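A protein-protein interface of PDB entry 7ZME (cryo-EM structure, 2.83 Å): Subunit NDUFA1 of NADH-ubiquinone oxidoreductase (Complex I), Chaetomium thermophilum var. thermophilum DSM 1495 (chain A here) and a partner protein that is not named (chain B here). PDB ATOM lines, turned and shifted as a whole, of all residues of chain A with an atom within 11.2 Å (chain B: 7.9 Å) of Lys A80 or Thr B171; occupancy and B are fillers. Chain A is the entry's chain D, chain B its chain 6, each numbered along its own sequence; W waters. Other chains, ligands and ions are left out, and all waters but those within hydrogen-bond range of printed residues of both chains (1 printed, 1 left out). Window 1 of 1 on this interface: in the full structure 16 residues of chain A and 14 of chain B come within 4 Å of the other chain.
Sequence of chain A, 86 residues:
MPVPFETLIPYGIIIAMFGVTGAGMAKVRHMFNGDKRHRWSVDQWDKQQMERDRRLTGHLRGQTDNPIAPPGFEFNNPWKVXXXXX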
ATOM      1  N   GLN A  44       4.644 -12.940  36.148  1.00  0.00           N
ATOM      2  CA  GLN A  44       5.252 -13.842  35.143  1.00  0.00           C
ATOM      3  C   GLN A  44       4.184 -14.686  34.447  1.00  0.00           C
ATOM      4  O   GLN A  44       4.297 -14.858  33.232  1.00  0.00           O
ATOM      5  CB  GLN A  44       6.382 -14.659  35.770  1.00  0.00           C
ATOM      6  CG  GLN A  44       7.157 -15.525  34.784  1.00  0.00           C
ATOM      7  CD  GLN A  44       7.743 -14.799  33.594  1.00  0.00           C
ATOM      8  OE1 GLN A  44       7.988 -15.392  32.548  1.00  0.00           O
ATOM      9  NE2 GLN A  44       7.989 -13.507  33.735  1.00  0.00           N
ATOM     10  N   LYS A  47       2.302 -12.628  31.858  1.00  0.00           N
ATOM     11  CA  LYS A  47       3.162 -12.197  30.738  1.00  0.00           C
ATOM     12  C   LYS A  47       3.396 -13.423  29.870  1.00  0.00           C
ATOM     13  O   LYS A  47       3.405 -13.258  28.643  1.00  0.00           O
ATOM     14  CB  LYS A  47       4.493 -11.711  31.313  1.00  0.00           C
ATOM     15  CG  LYS A  47       4.471 -10.378  32.043  1.00  0.00           C
ATOM     16  CD  LYS A  47       5.813 -10.043  32.659  1.00  0.00           C
ATOM     17  CE  LYS A  47       5.830  -8.718  33.389  1.00  0.00           C
ATOM     18  NZ  LYS A  47       4.974  -8.744  34.598  1.00  0.00           N
ATOM     19  N   GLN A  48       3.545 -14.596  30.482  1.00  0.00           N
ATOM     20  CA  GLN A  48       3.651 -15.874  29.736  1.00  0.00           C
ATOM     21  C   GLN A  48       2.341 -16.202  29.024  1.00  0.00           C
ATOM     22  O   GLN A  48       2.414 -16.827  27.967  1.00  0.00           O
ATOM     23  CB  GLN A  48       4.055 -16.980  30.706  1.00  0.00           C
ATOM     24  CG  GLN A  48       5.507 -16.965  31.134  1.00  0.00           C
ATOM     25  CD  GLN A  48       5.784 -18.179  31.983  1.00  0.00           C
ATOM     26  OE1 GLN A  48       4.958 -19.077  32.087  1.00  0.00           O
ATOM     27  NE2 GLN A  48       6.957 -18.220  32.587  1.00  0.00           N
ATOM     28  N   GLN A  49       1.201 -15.804  29.579  1.00  0.00           N
ATOM     29  CA  GLN A  49      -0.130 -16.102  28.983  1.00  0.00           C
ATOM     30  C   GLN A  49      -0.391 -15.164  27.803  1.00  0.00           C
ATOM     31  O   GLN A  49      -1.027 -15.604  26.847  1.00  0.00           O
ATOM     32  CB  GLN A  49      -1.215 -16.044  30.054  1.00  0.00           C
ATOM     33  CG  GLN A  49      -1.241 -17.245  30.986  1.00  0.00           C
ATOM     34  CD  GLN A  49      -1.826 -18.501  30.388  1.00  0.00           C
ATOM     35  OE1 GLN A  49      -2.224 -18.550  29.229  1.00  0.00           O
ATOM     36  NE2 GLN A  49      -1.893 -19.544  31.196  1.00  0.00           N
ATOM     37  N   MET A  50       0.056 -13.911  27.892  1.00  0.00           N
ATOM     38  CA  MET A  50      -0.081 -12.939  26.778  1.00  0.00           C
ATOM     39  C   MET A  50       0.812 -13.365  25.617  1.00  0.00           C
ATOM     40  O   MET A  50       0.410 -13.159  24.467  1.00  0.00           O
ATOM     41  CB  MET A  50       0.225 -11.508  27.229  1.00  0.00           C
ATOM     42  CG  MET A  50      -0.940 -10.881  27.968  1.00  0.00           C
ATOM     43  SD  MET A  50      -0.661  -9.204  28.573  1.00  0.00           S
ATOM     44  CE  MET A  50       0.683  -9.477  29.724  1.00  0.00           C
ATOM     45  N   GLU A  51       1.960 -13.973  25.915  1.00  0.00           N
ATOM     46  CA  GLU A  51       2.915 -14.359  24.854  1.00  0.00           C
ATOM     47  C   GLU A  51       2.371 -15.628  24.211  1.00  0.00           C
ATOM     48  O   GLU A  51       2.605 -15.812  23.009  1.00  0.00           O
ATOM     49  CB  GLU A  51       4.286 -14.597  25.475  1.00  0.00           C
ATOM     50  CG  GLU A  51       5.083 -13.325  25.678  1.00  0.00           C
ATOM     51  CD  GLU A  51       6.247 -13.485  26.639  1.00  0.00           C
ATOM     52  OE1 GLU A  51       6.259 -14.487  27.381  1.00  0.00           O
ATOM     53  OE2 GLU A  51       7.135 -12.609  26.641  1.00  0.00           O
ATOM     54  N   ARG A  52       1.657 -16.447  24.979  1.00  0.00           N
ATOM     55  CA  ARG A  52       0.982 -17.632  24.397  1.00  0.00           C
ATOM     56  C   ARG A  52      -0.159 -17.175  23.479  1.00  0.00           C
ATOM     57  O   ARG A  52      -0.403 -17.847  22.478  1.00  0.00           O
ATOM     58  CB  ARG A  52       0.627 -18.648  25.486  1.00  0.00           C
ATOM     59  CG  ARG A  52       0.228 -20.006  24.930  1.00  0.00           C
ATOM     60  CD  ARG A  52      -0.025 -21.081  25.965  1.00  0.00           C
ATOM     61  NE  ARG A  52      -0.635 -22.236  25.327  1.00  0.00           N
ATOM     62  CZ  ARG A  52      -1.941 -22.458  25.273  1.00  0.00           C
ATOM     63  NH1 ARG A  52      -2.781 -21.615  25.845  1.00  0.00           N
ATOM     64  NH2 ARG A  52      -2.404 -23.530  24.659  1.00  0.00           N
ATOM     65  N   ASP A  53      -0.860 -16.106  23.832  1.00  0.00           N
ATOM     66  CA  ASP A  53      -1.961 -15.547  22.994  1.00  0.00           C
ATOM     67  C   ASP A  53      -1.433 -15.035  21.647  1.00  0.00           C
ATOM     68  O   ASP A  53      -2.126 -15.226  20.647  1.00  0.00           O
ATOM     69  CB  ASP A  53      -2.699 -14.429  23.734  1.00  0.00           C
ATOM     70  CG  ASP A  53      -3.546 -14.906  24.894  1.00  0.00           C
ATOM     71  OD1 ASP A  53      -3.679 -16.128  25.056  1.00  0.00           O
ATOM     72  OD2 ASP A  53      -4.064 -14.048  25.625  1.00  0.00           O
ATOM     73  N   ARG A  54      -0.273 -14.376  21.630  1.00  0.00           N
ATOM     74  CA  ARG A  54       0.362 -13.909  20.371  1.00  0.00           C
ATOM     75  C   ARG A  54       0.700 -15.139  19.530  1.00  0.00           C
ATOM     76  O   ARG A  54       0.585 -15.063  18.305  1.00  0.00           O
ATOM     77  CB  ARG A  54       1.579 -13.035  20.684  1.00  0.00           C
ATOM     78  CG  ARG A  54       2.119 -12.262  19.492  1.00  0.00           C
ATOM     79  CD  ARG A  54       3.619 -12.064  19.488  1.00  0.00           C
ATOM     80  NE  ARG A  54       4.087 -10.838  20.118  1.00  0.00           N
ATOM     81  CZ  ARG A  54       4.871 -10.796  21.185  1.00  0.00           C
ATOM     82  NH1 ARG A  54       5.257  -9.631  21.675  1.00  0.00           N
ATOM     83  NH2 ARG A  54       5.273 -11.917  21.753  1.00  0.00           N
ATOM     84  N   ARG A  55       1.092 -16.237  20.173  1.00  0.00           N
ATOM     85  CA  ARG A  55       1.396 -17.501  19.462  1.00  0.00           C
ATOM     86  C   ARG A  55       0.160 -18.008  18.707  1.00  0.00           C
ATOM     87  O   ARG A  55       0.347 -18.612  17.643  1.00  0.00           O
ATOM     88  CB  ARG A  55       1.948 -18.536  20.441  1.00  0.00           C
ATOM     89  CG  ARG A  55       3.370 -18.283  20.909  1.00  0.00           C
ATOM     90  CD  ARG A  55       3.731 -19.336  21.933  1.00  0.00           C
ATOM     91  NE  ARG A  55       3.740 -20.668  21.352  1.00  0.00           N
ATOM     92  CZ  ARG A  55       3.736 -21.791  22.056  1.00  0.00           C
ATOM     93  NH1 ARG A  55       3.704 -21.742  23.376  1.00  0.00           N
ATOM     94  NH2 ARG A  55       3.753 -22.958  21.439  1.00  0.00           N
ATOM     95  N   LEU A  60      -0.847  -9.899  21.422  1.00  0.00           N
ATOM     96  CA  LEU A  60      -0.607 -10.294  22.839  1.00  0.00           C
ATOM     97  C   LEU A  60      -1.921 -10.330  23.611  1.00  0.00           C
ATOM     98  O   LEU A  60      -1.995 -11.049  24.602  1.00  0.00           O
ATOM     99  CB  LEU A  60       0.359  -9.297  23.481  1.00  0.00           C
ATOM    100  CG  LEU A  60       1.824  -9.412  23.079  1.00  0.00           C
ATOM    101  CD1 LEU A  60       2.515  -8.065  23.227  1.00  0.00           C
ATOM    102  CD2 LEU A  60       2.519 -10.467  23.919  1.00  0.00           C
ATOM    103  N   PHE A  75       6.007 -25.207  16.798  1.00  0.00           N
ATOM    104  CA  PHE A  75       7.305 -24.613  16.399  1.00  0.00           C
ATOM    105  C   PHE A  75       7.364 -23.106  16.665  1.00  0.00           C
ATOM    106  O   PHE A  75       8.454 -22.551  16.492  1.00  0.00           O
ATOM    107  CB  PHE A  75       7.491 -24.817  14.899  1.00  0.00           C
ATOM    108  CG  PHE A  75       7.237 -26.216  14.402  1.00  0.00           C
ATOM    109  CD1 PHE A  75       8.208 -27.194  14.518  1.00  0.00           C
ATOM    110  CD2 PHE A  75       6.034 -26.548  13.805  1.00  0.00           C
ATOM    111  CE1 PHE A  75       7.978 -28.476  14.052  1.00  0.00           C
ATOM    112  CE2 PHE A  75       5.809 -27.829  13.331  1.00  0.00           C
ATOM    113  CZ  PHE A  75       6.780 -28.792  13.459  1.00  0.00           C
ATOM    114  N   ASN A  76       6.274 -22.466  17.101  1.00  0.00           N
ATOM    115  CA  ASN A  76       6.264 -20.978  17.241  1.00  0.00           C
ATOM    116  C   ASN A  76       6.576 -20.543  18.672  1.00  0.00           C
ATOM    117  O   ASN A  76       6.369 -19.365  18.967  1.00  0.00           O
ATOM    118  CB  ASN A  76       5.005 -20.311  16.662  1.00  0.00           C
ATOM    119  CG  ASN A  76       3.715 -20.565  17.411  1.00  0.00           C
ATOM    120  OD1 ASN A  76       3.709 -21.088  18.518  1.00  0.00           O
ATOM    121  ND2 ASN A  76       2.604 -20.170  16.816  1.00  0.00           N
ATOM    122  N   ASN A  77       7.078 -21.450  19.509  1.00  0.00           N
ATOM    123  CA  ASN A  77       7.290 -21.101  20.937  1.00  0.00           C
ATOM    124  C   ASN A  77       8.542 -20.228  21.005  1.00  0.00           C
ATOM    125  O   ASN A  77       9.609 -20.692  20.582  1.00  0.00           O
ATOM    126  CB  ASN A  77       7.393 -22.320  21.851  1.00  0.00           C
ATOM    127  CG  ASN A  77       7.294 -21.985  23.322  1.00  0.00           C
ATOM    128  OD1 ASN A  77       6.826 -20.913  23.693  1.00  0.00           O
ATOM    129  ND2 ASN A  77       7.716 -22.906  24.170  1.00  0.00           N
ATOM    130  N   PRO A  78       8.458 -18.946  21.429  1.00  0.00           N
ATOM    131  CA  PRO A  78       9.618 -18.051  21.401  1.00  0.00           C
ATOM    132  C   PRO A  78      10.570 -18.370  22.542  1.00  0.00           C
ATOM    133  O   PRO A  78      10.153 -18.521  23.692  1.00  0.00           O
ATOM    134  CB  PRO A  78       8.997 -16.656  21.563  1.00  0.00           C
ATOM    135  CG  PRO A  78       7.507 -16.862  21.485  1.00  0.00           C
ATOM    136  CD  PRO A  78       7.271 -18.258  21.948  1.00  0.00           C
ATOM    137  N   TRP A  79      11.848 -18.482  22.217  1.00  0.00           N
ATOM    138  CA  TRP A  79      12.896 -18.592  23.217  1.00  0.00           C
ATOM    139  C   TRP A  79      13.687 -17.292  23.201  1.00  0.00           C
ATOM    140  O   TRP A  79      14.284 -16.939  22.182  1.00  0.00           O
ATOM    141  CB  TRP A  79      13.790 -19.800  22.948  1.00  0.00           C
ATOM    142  CG  TRP A  79      13.231 -21.059  23.521  1.00  0.00           C
ATOM    143  CD1 TRP A  79      11.946 -21.276  23.902  1.00  0.00           C
ATOM    144  CD2 TRP A  79      13.938 -22.275  23.785  1.00  0.00           C
ATOM    145  NE1 TRP A  79      11.801 -22.549  24.385  1.00  0.00           N
ATOM    146  CE2 TRP A  79      13.011 -23.186  24.323  1.00  0.00           C
ATOM    147  CE3 TRP A  79      15.266 -22.682  23.616  1.00  0.00           C
ATOM    148  CZ2 TRP A  79      13.366 -24.475  24.695  1.00  0.00           C
ATOM    149  CZ3 TRP A  79      15.615 -23.964  23.987  1.00  0.00           C
ATOM    150  CH2 TRP A  79      14.668 -24.845  24.521  1.00  0.00           C
ATOM    151  N   LYS A  80      13.676 -16.582  24.325  1.00  0.00           N
ATOM    152  CA  LYS A  80      14.251 -15.248  24.372  1.00  0.00           C
ATOM    153  C   LYS A  80      15.767 -15.320  24.259  1.00  0.00           C
ATOM    154  O   LYS A  80      16.416 -16.146  24.901  1.00  0.00           O
ATOM    155  CB  LYS A  80      13.863 -14.547  25.671  1.00  0.00           C
ATOM    156  CG  LYS A  80      12.376 -14.430  25.913  1.00  0.00           C
ATOM    157  CD  LYS A  80      11.668 -13.708  24.806  1.00  0.00           C
ATOM    158  CE  LYS A  80      10.170 -13.791  25.009  1.00  0.00           C
ATOM    159  NZ  LYS A  80       9.532 -14.717  24.042  1.00  0.00           N
ATOM    160  N   VAL A  81      16.333 -14.436  23.447  1.00  0.00           N
ATOM    161  CA  VAL A  81      17.764 -14.415  23.180  1.00  0.00           C
ATOM    162  C   VAL A  81      18.318 -13.096  23.695  1.00  0.00           C
ATOM    163  O   VAL A  81      17.861 -12.021  23.288  1.00  0.00           O
ATOM    164  CB  VAL A  81      18.063 -14.590  21.685  1.00  0.00           C
ATOM    165  CG1 VAL A  81      19.542 -14.721  21.461  1.00  0.00           C
ATOM    166  CG2 VAL A  81      17.335 -15.798  21.140  1.00  0.00           C
ATOM    167  N   UNK A  82      19.293 -13.176  24.593  1.00  0.00           N
ATOM    168  CA  UNK A  82      19.940 -12.007  25.163  1.00  0.00           C
ATOM    169  C   UNK A  82      21.447 -12.119  24.991  1.00  0.00           C
ATOM    170  O   UNK A  82      21.984 -13.180  24.672  1.00  0.00           O
ATOM    171  CB  UNK A  82      19.590 -11.832  26.647  1.00  0.00           C
ATOM    172  N   UNK A  83      22.130 -10.998  25.206  1.00  0.00           N
ATOM    173  CA  UNK A  83      23.581 -10.966  25.103  1.00  0.00           C
ATOM    174  C   UNK A  83      24.291 -10.939  26.447  1.00  0.00           C
ATOM    175  O   UNK A  83      25.354 -11.556  26.573  1.00  0.00           O
ATOM    176  CB  UNK A  83      24.030  -9.755  24.278  1.00  0.00           C
ATOM    177  N   UNK A  84      23.704 -10.305  27.476  1.00  0.00           N
ATOM    178  CA  UNK A  84      24.489 -10.165  28.728  1.00  0.00           C
ATOM    179  C   UNK A  84      23.789 -10.518  30.042  1.00  0.00           C
ATOM    180  O   UNK A  84      24.491 -11.056  30.918  1.00  0.00           O
ATOM    181  CB  UNK A  84      25.083  -8.773  28.807  1.00  0.00           C
ATOM    182  N   UNK A  85      22.487 -10.275  30.194  1.00  0.00           N
ATOM    183  CA  UNK A  85      21.865 -10.409  31.537  1.00  0.00           C
ATOM    184  C   UNK A  85      21.463 -11.817  31.954  1.00  0.00           C
ATOM    185  O   UNK A  85      20.258 -12.028  32.126  1.00  0.00           O
ATOM    186  CB  UNK A  85      20.670  -9.525  31.622  1.00  0.00           C
ATOM    187  N   UNK A  86      22.424 -12.710  32.163  1.00  0.00           N
ATOM    188  CA  UNK A  86      22.101 -14.025  32.739  1.00  0.00           C
ATOM    189  C   UNK A  86      22.484 -13.983  34.219  1.00  0.00           C
ATOM    190  O   UNK A  86      22.067 -13.004  34.872  1.00  0.00           O
ATOM    191  CB  UNK A  86      22.855 -15.097  32.011  1.00  0.00           C
ATOM    192  N   LEU B   9      16.531 -16.690  13.496  1.00  0.00           N
ATOM    193  CA  LEU B   9      16.700 -15.556  14.429  1.00  0.00           C
ATOM    194  C   LEU B   9      15.656 -14.518  14.041  1.00  0.00           C
ATOM    195  O   LEU B   9      15.355 -14.399  12.851  1.00  0.00           O
ATOM    196  CB  LEU B   9      18.129 -15.010  14.406  1.00  0.00           C
ATOM    197  CG  LEU B   9      18.531 -14.177  15.621  1.00  0.00           C
ATOM    198  CD1 LEU B   9      18.229 -14.917  16.913  1.00  0.00           C
ATOM    199  CD2 LEU B   9      20.003 -13.807  15.553  1.00  0.00           C
ATOM    200  N   GLU B  12      12.403  -9.254  18.441  1.00  0.00           N
ATOM    201  CA  GLU B  12      11.228  -9.202  19.301  1.00  0.00           C
ATOM    202  C   GLU B  12      10.544  -7.849  19.138  1.00  0.00           C
ATOM    203  O   GLU B  12      11.145  -6.808  19.414  1.00  0.00           O
ATOM    204  CB  GLU B  12      11.639  -9.438  20.751  1.00  0.00           C
ATOM    205  CG  GLU B  12      10.545 -10.009  21.623  1.00  0.00           C
ATOM    206  CD  GLU B  12      11.072 -10.524  22.942  1.00  0.00           C
ATOM    207  OE1 GLU B  12      10.253 -10.865  23.819  1.00  0.00           O
ATOM    208  OE2 GLU B  12      12.309 -10.589  23.100  1.00  0.00           O
ATOM    209  N   TYR B  14       7.390  -6.510  20.446  1.00  0.00           N
ATOM    210  CA  TYR B  14       7.081  -5.996  21.770  1.00  0.00           C
ATOM    211  C   TYR B  14       7.699  -6.933  22.796  1.00  0.00           C
ATOM    212  O   TYR B  14       8.347  -7.922  22.451  1.00  0.00           O
ATOM    213  CB  TYR B  14       5.570  -5.865  21.987  1.00  0.00           C
ATOM    214  CG  TYR B  14       4.856  -4.997  20.975  1.00  0.00           C
ATOM    215  CD1 TYR B  14       4.431  -5.513  19.762  1.00  0.00           C
ATOM    216  CD2 TYR B  14       4.596  -3.661  21.242  1.00  0.00           C
ATOM    217  CE1 TYR B  14       3.779  -4.723  18.841  1.00  0.00           C
ATOM    218  CE2 TYR B  14       3.943  -2.865  20.326  1.00  0.00           C
ATOM    219  CZ  TYR B  14       3.536  -3.400  19.128  1.00  0.00           C
ATOM    220  OH  TYR B  14       2.883  -2.604  18.216  1.00  0.00           O
ATOM    221  N   THR B  15       7.503  -6.615  24.070  1.00  0.00           N
ATOM    222  CA  THR B  15       7.934  -7.444  25.191  1.00  0.00           C
ATOM    223  C   THR B  15       9.447  -7.644  25.231  1.00  0.00           C
ATOM    224  O   THR B  15       9.946  -8.396  26.077  1.00  0.00           O
ATOM    225  CB  THR B  15       7.227  -8.809  25.197  1.00  0.00           C
ATOM    226  OG1 THR B  15       7.546  -9.531  24.002  1.00  0.00           O
ATOM    227  CG2 THR B  15       5.721  -8.624  25.268  1.00  0.00           C
ATOM    228  N   ASN B  16      10.189  -6.994  24.341  1.00  0.00           N
ATOM    229  CA  ASN B  16      11.638  -7.033  24.398  1.00  0.00           C
ATOM    230  C   ASN B  16      12.148  -6.225  25.588  1.00  0.00           C
ATOM    231  O   ASN B  16      11.463  -5.350  26.125  1.00  0.00           O
ATOM    232  CB  ASN B  16      12.240  -6.511  23.094  1.00  0.00           C
ATOM    233  CG  ASN B  16      11.761  -5.122  22.739  1.00  0.00           C
ATOM    234  OD1 ASN B  16      11.009  -4.497  23.483  1.00  0.00           O
ATOM    235  ND2 ASN B  16      12.201  -4.627  21.593  1.00  0.00           N
ATOM    236  N   GLY B  17      13.368  -6.533  26.003  1.00  0.00           N
ATOM    237  CA  GLY B  17      13.965  -5.929  27.171  1.00  0.00           C
ATOM    238  C   GLY B  17      14.696  -4.648  26.850  1.00  0.00           C
ATOM    239  O   GLY B  17      14.523  -4.046  25.789  1.00  0.00           O
ATOM    240  N   PHE B 168      25.121 -16.351  23.079  1.00  0.00           N
ATOM    241  CA  PHE B 168      23.833 -15.679  23.372  1.00  0.00           C
ATOM    242  C   PHE B 168      23.105 -16.469  24.452  1.00  0.00           C
ATOM    243  O   PHE B 168      23.002 -17.701  24.344  1.00  0.00           O
ATOM    244  CB  PHE B 168      22.983 -15.543  22.110  1.00  0.00           C
ATOM    245  CG  PHE B 168      23.512 -14.524  21.134  1.00  0.00           C
ATOM    246  CD1 PHE B 168      23.196 -13.183  21.272  1.00  0.00           C
ATOM    247  CD2 PHE B 168      24.347 -14.901  20.096  1.00  0.00           C
ATOM    248  CE1 PHE B 168      23.693 -12.244  20.385  1.00  0.00           C
ATOM    249  CE2 PHE B 168      24.842 -13.960  19.209  1.00  0.00           C
ATOM    250  CZ  PHE B 168      24.514 -12.633  19.354  1.00  0.00           C
ATOM    251  N   PHE B 169      22.665 -15.765  25.490  1.00  0.00           N
ATOM    252  CA  PHE B 169      21.897 -16.412  26.577  1.00  0.00           C
ATOM    253  C   PHE B 169      20.491 -16.725  26.085  1.00  0.00           C
ATOM    254  O   PHE B 169      19.884 -15.889  25.418  1.00  0.00           O
ATOM    255  CB  PHE B 169      21.934 -15.537  27.826  1.00  0.00           C
ATOM    256  CG  PHE B 169      23.303 -15.371  28.432  1.00  0.00           C
ATOM    257  CD1 PHE B 169      23.887 -16.400  29.147  1.00  0.00           C
ATOM    258  CD2 PHE B 169      24.001 -14.187  28.288  1.00  0.00           C
ATOM    259  CE1 PHE B 169      25.145 -16.243  29.706  1.00  0.00           C
ATOM    260  CE2 PHE B 169      25.260 -14.034  28.845  1.00  0.00           C
ATOM    261  CZ  PHE B 169      25.830 -15.064  29.552  1.00  0.00           C
ATOM    262  N   ILE B 170      19.997 -17.908  26.423  1.00  0.00           N
ATOM    263  CA  ILE B 170      18.653 -18.358  25.956  1.00  0.00           C
ATOM    264  C   ILE B 170      17.758 -18.592  27.177  1.00  0.00           C
ATOM    265  O   ILE B 170      18.222 -19.224  28.133  1.00  0.00           O
ATOM    266  CB  ILE B 170      18.774 -19.574  25.015  1.00  0.00           C
ATOM    267  CG1 ILE B 170      17.491 -19.813  24.218  1.00  0.00           C
ATOM    268  CG2 ILE B 170      19.242 -20.824  25.737  1.00  0.00           C
ATOM    269  CD1 ILE B 170      17.329 -18.893  23.040  1.00  0.00           C
ATOM    270  N   THR B 171      16.549 -18.033  27.170  1.00  0.00           N
ATOM    271  CA  THR B 171      15.605 -18.248  28.256  1.00  0.00           C
ATOM    272  C   THR B 171      14.268 -18.712  27.700  1.00  0.00           C
ATOM    273  O   THR B 171      13.846 -18.299  26.619  1.00  0.00           O
ATOM    274  CB  THR B 171      15.382 -16.988  29.111  1.00  0.00           C
ATOM    275  OG1 THR B 171      14.620 -16.029  28.370  1.00  0.00           O
ATOM    276  CG2 THR B 171      16.701 -16.374  29.533  1.00  0.00           C
ATOM    277  N   SER B 172      13.572 -19.560  28.461  1.00  0.00           N
ATOM    278  CA  SER B 172      12.227 -20.053  28.069  1.00  0.00           C
ATOM    279  C   SER B 172      11.284 -19.858  29.255  1.00  0.00           C
ATOM    280  O   SER B 172      11.676 -19.153  30.192  1.00  0.00           O
ATOM    281  CB  SER B 172      12.264 -21.482  27.628  1.00  0.00           C
ATOM    282  OG  SER B 172      12.484 -22.342  28.728  1.00  0.00           O
ATOM    283  N   LYS B 173      10.111 -20.493  29.239  1.00  0.00           N
ATOM    284  CA  LYS B 173       9.108 -20.239  30.306  1.00  0.00           C
ATOM    285  C   LYS B 173       8.767 -21.501  31.111  1.00  0.00           C
ATOM    286  O   LYS B 173       8.967 -22.596  30.576  1.00  0.00           O
ATOM    287  CB  LYS B 173       7.877 -19.642  29.627  1.00  0.00           C
ATOM    288  CG  LYS B 173       6.997 -20.599  28.840  1.00  0.00           C
ATOM    289  CD  LYS B 173       5.783 -19.922  28.256  1.00  0.00           C
ATOM    290  CE  LYS B 173       6.127 -18.719  27.405  1.00  0.00           C
ATOM    291  NZ  LYS B 173       4.911 -18.066  26.869  1.00  0.00           N
HETATM  292  O   HOH W   1      16.880 -14.203  27.082  1.00  0.00           O
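The side-chain carboxylate (OE1) of Glu B12 lies within salt-bridge range of the side-chain amino group (NZ) of Lys A80 (3.9 Å).
O of UNK A82 lies within hydrogen-bond range of the backbone NH of Phe B169 (2.8 Å).
NZ of Lys B173 lies within salt-bridge range of OE1 of Glu A51 (3.9 Å).
The backbone NH of Lys A80 sits at hydrogen-bond distance from the backbone carbonyl oxygen of Thr B171, 2.9 Å away.
The side-chain amino group of Lys B173 sits at hydrogen-bond distance from the backbone carbonyl oxygen of Gln A48 (3.0 Å).
The guanidinium group (NH1) of Arg A54 is in hydrogen-bond range of the side-chain hydroxyl (OG1) of Thr B15, 3.3 Å away.
The side-chain amide nitrogen (ND2) of Asn B16 lies within hydrogen-bond range of the backbone carbonyl oxygen (O) of Glu B12, 3.3 Å away.
OE1 of Gln A44 is in hydrogen-bond range of NE2 of Gln A48 (3.0 Å).
OG1 of Thr B15 lies within hydrogen-bond range of OE1 of Glu B12 (3.0 Å).
Tyr B14 touches Arg A54 (O to NH1, 3.6 Å).
Leu A60 touches Thr B15 (CD1 to CG2, 3.8 Å).
Ile B170 touches Trp A79.
O of Thr B171 touches CA of Trp A79 (3.5 Å).
CB of Ser B172 touches NE1 of Trp A79, 3.4 Å away.
Lys A80 touches Phe B169 (O to O, 3.5 Å).
Val A81 touches Phe B168 (CG1 to CB, 3.6 Å).
Val A81 touches Phe B169 (CA to O, 3.4 Å).
CG2 of Val A81 touches CD1 of Ile B170, 3.6 Å away.
Phe B168 touches UNK A82.
Of chain B, only Glu B12 (3.2 Å), Phe B169 (3.5 Å), Ile B170 (3.3 Å) and Thr B171 (2.9 Å) come within 4 Å of Lys A80.
Thr B171 touches just these residues of chain A: Trp A79 and Lys A80.
Ile B170 touches just these residues of chain A: Trp A79 (3.7 Å), Lys A80 (3.3 Å) and Val A81 (3.6 Å).
Of the printed residues of chain A, Ser B172 touches Trp A79 (3.4 Å).
Of the printed residues of chain B, UNK A84 touches Phe B169 (3.7 Å).
Of the printed residues of chain B, Gln A48 touches Lys B173 (3.0 Å).
Of the printed residues of chain B, UNK A86 touches Phe B169.
Of the printed residues of chain B, UNK A83 touches Phe B169.
Of the printed residues of chain A, Thr B15 touches Arg A54 and Leu A60.
Gly B17 touches none of the printed residues of chain A.
Arg A52 touches none of the printed residues of chain B.
The nearest residue of chain A that does not touch Thr B171 is Pro A78 (4.7 Å).
Along chain B the printed residues that touch a printed residue of chain A span positions 12 to 173.
Among the printed residues, 21 pairs touch across the chains.
Water W1 bridges the backbone carbonyl oxygen of Lys A80 and the side-chain hydroxyl of Thr B171.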
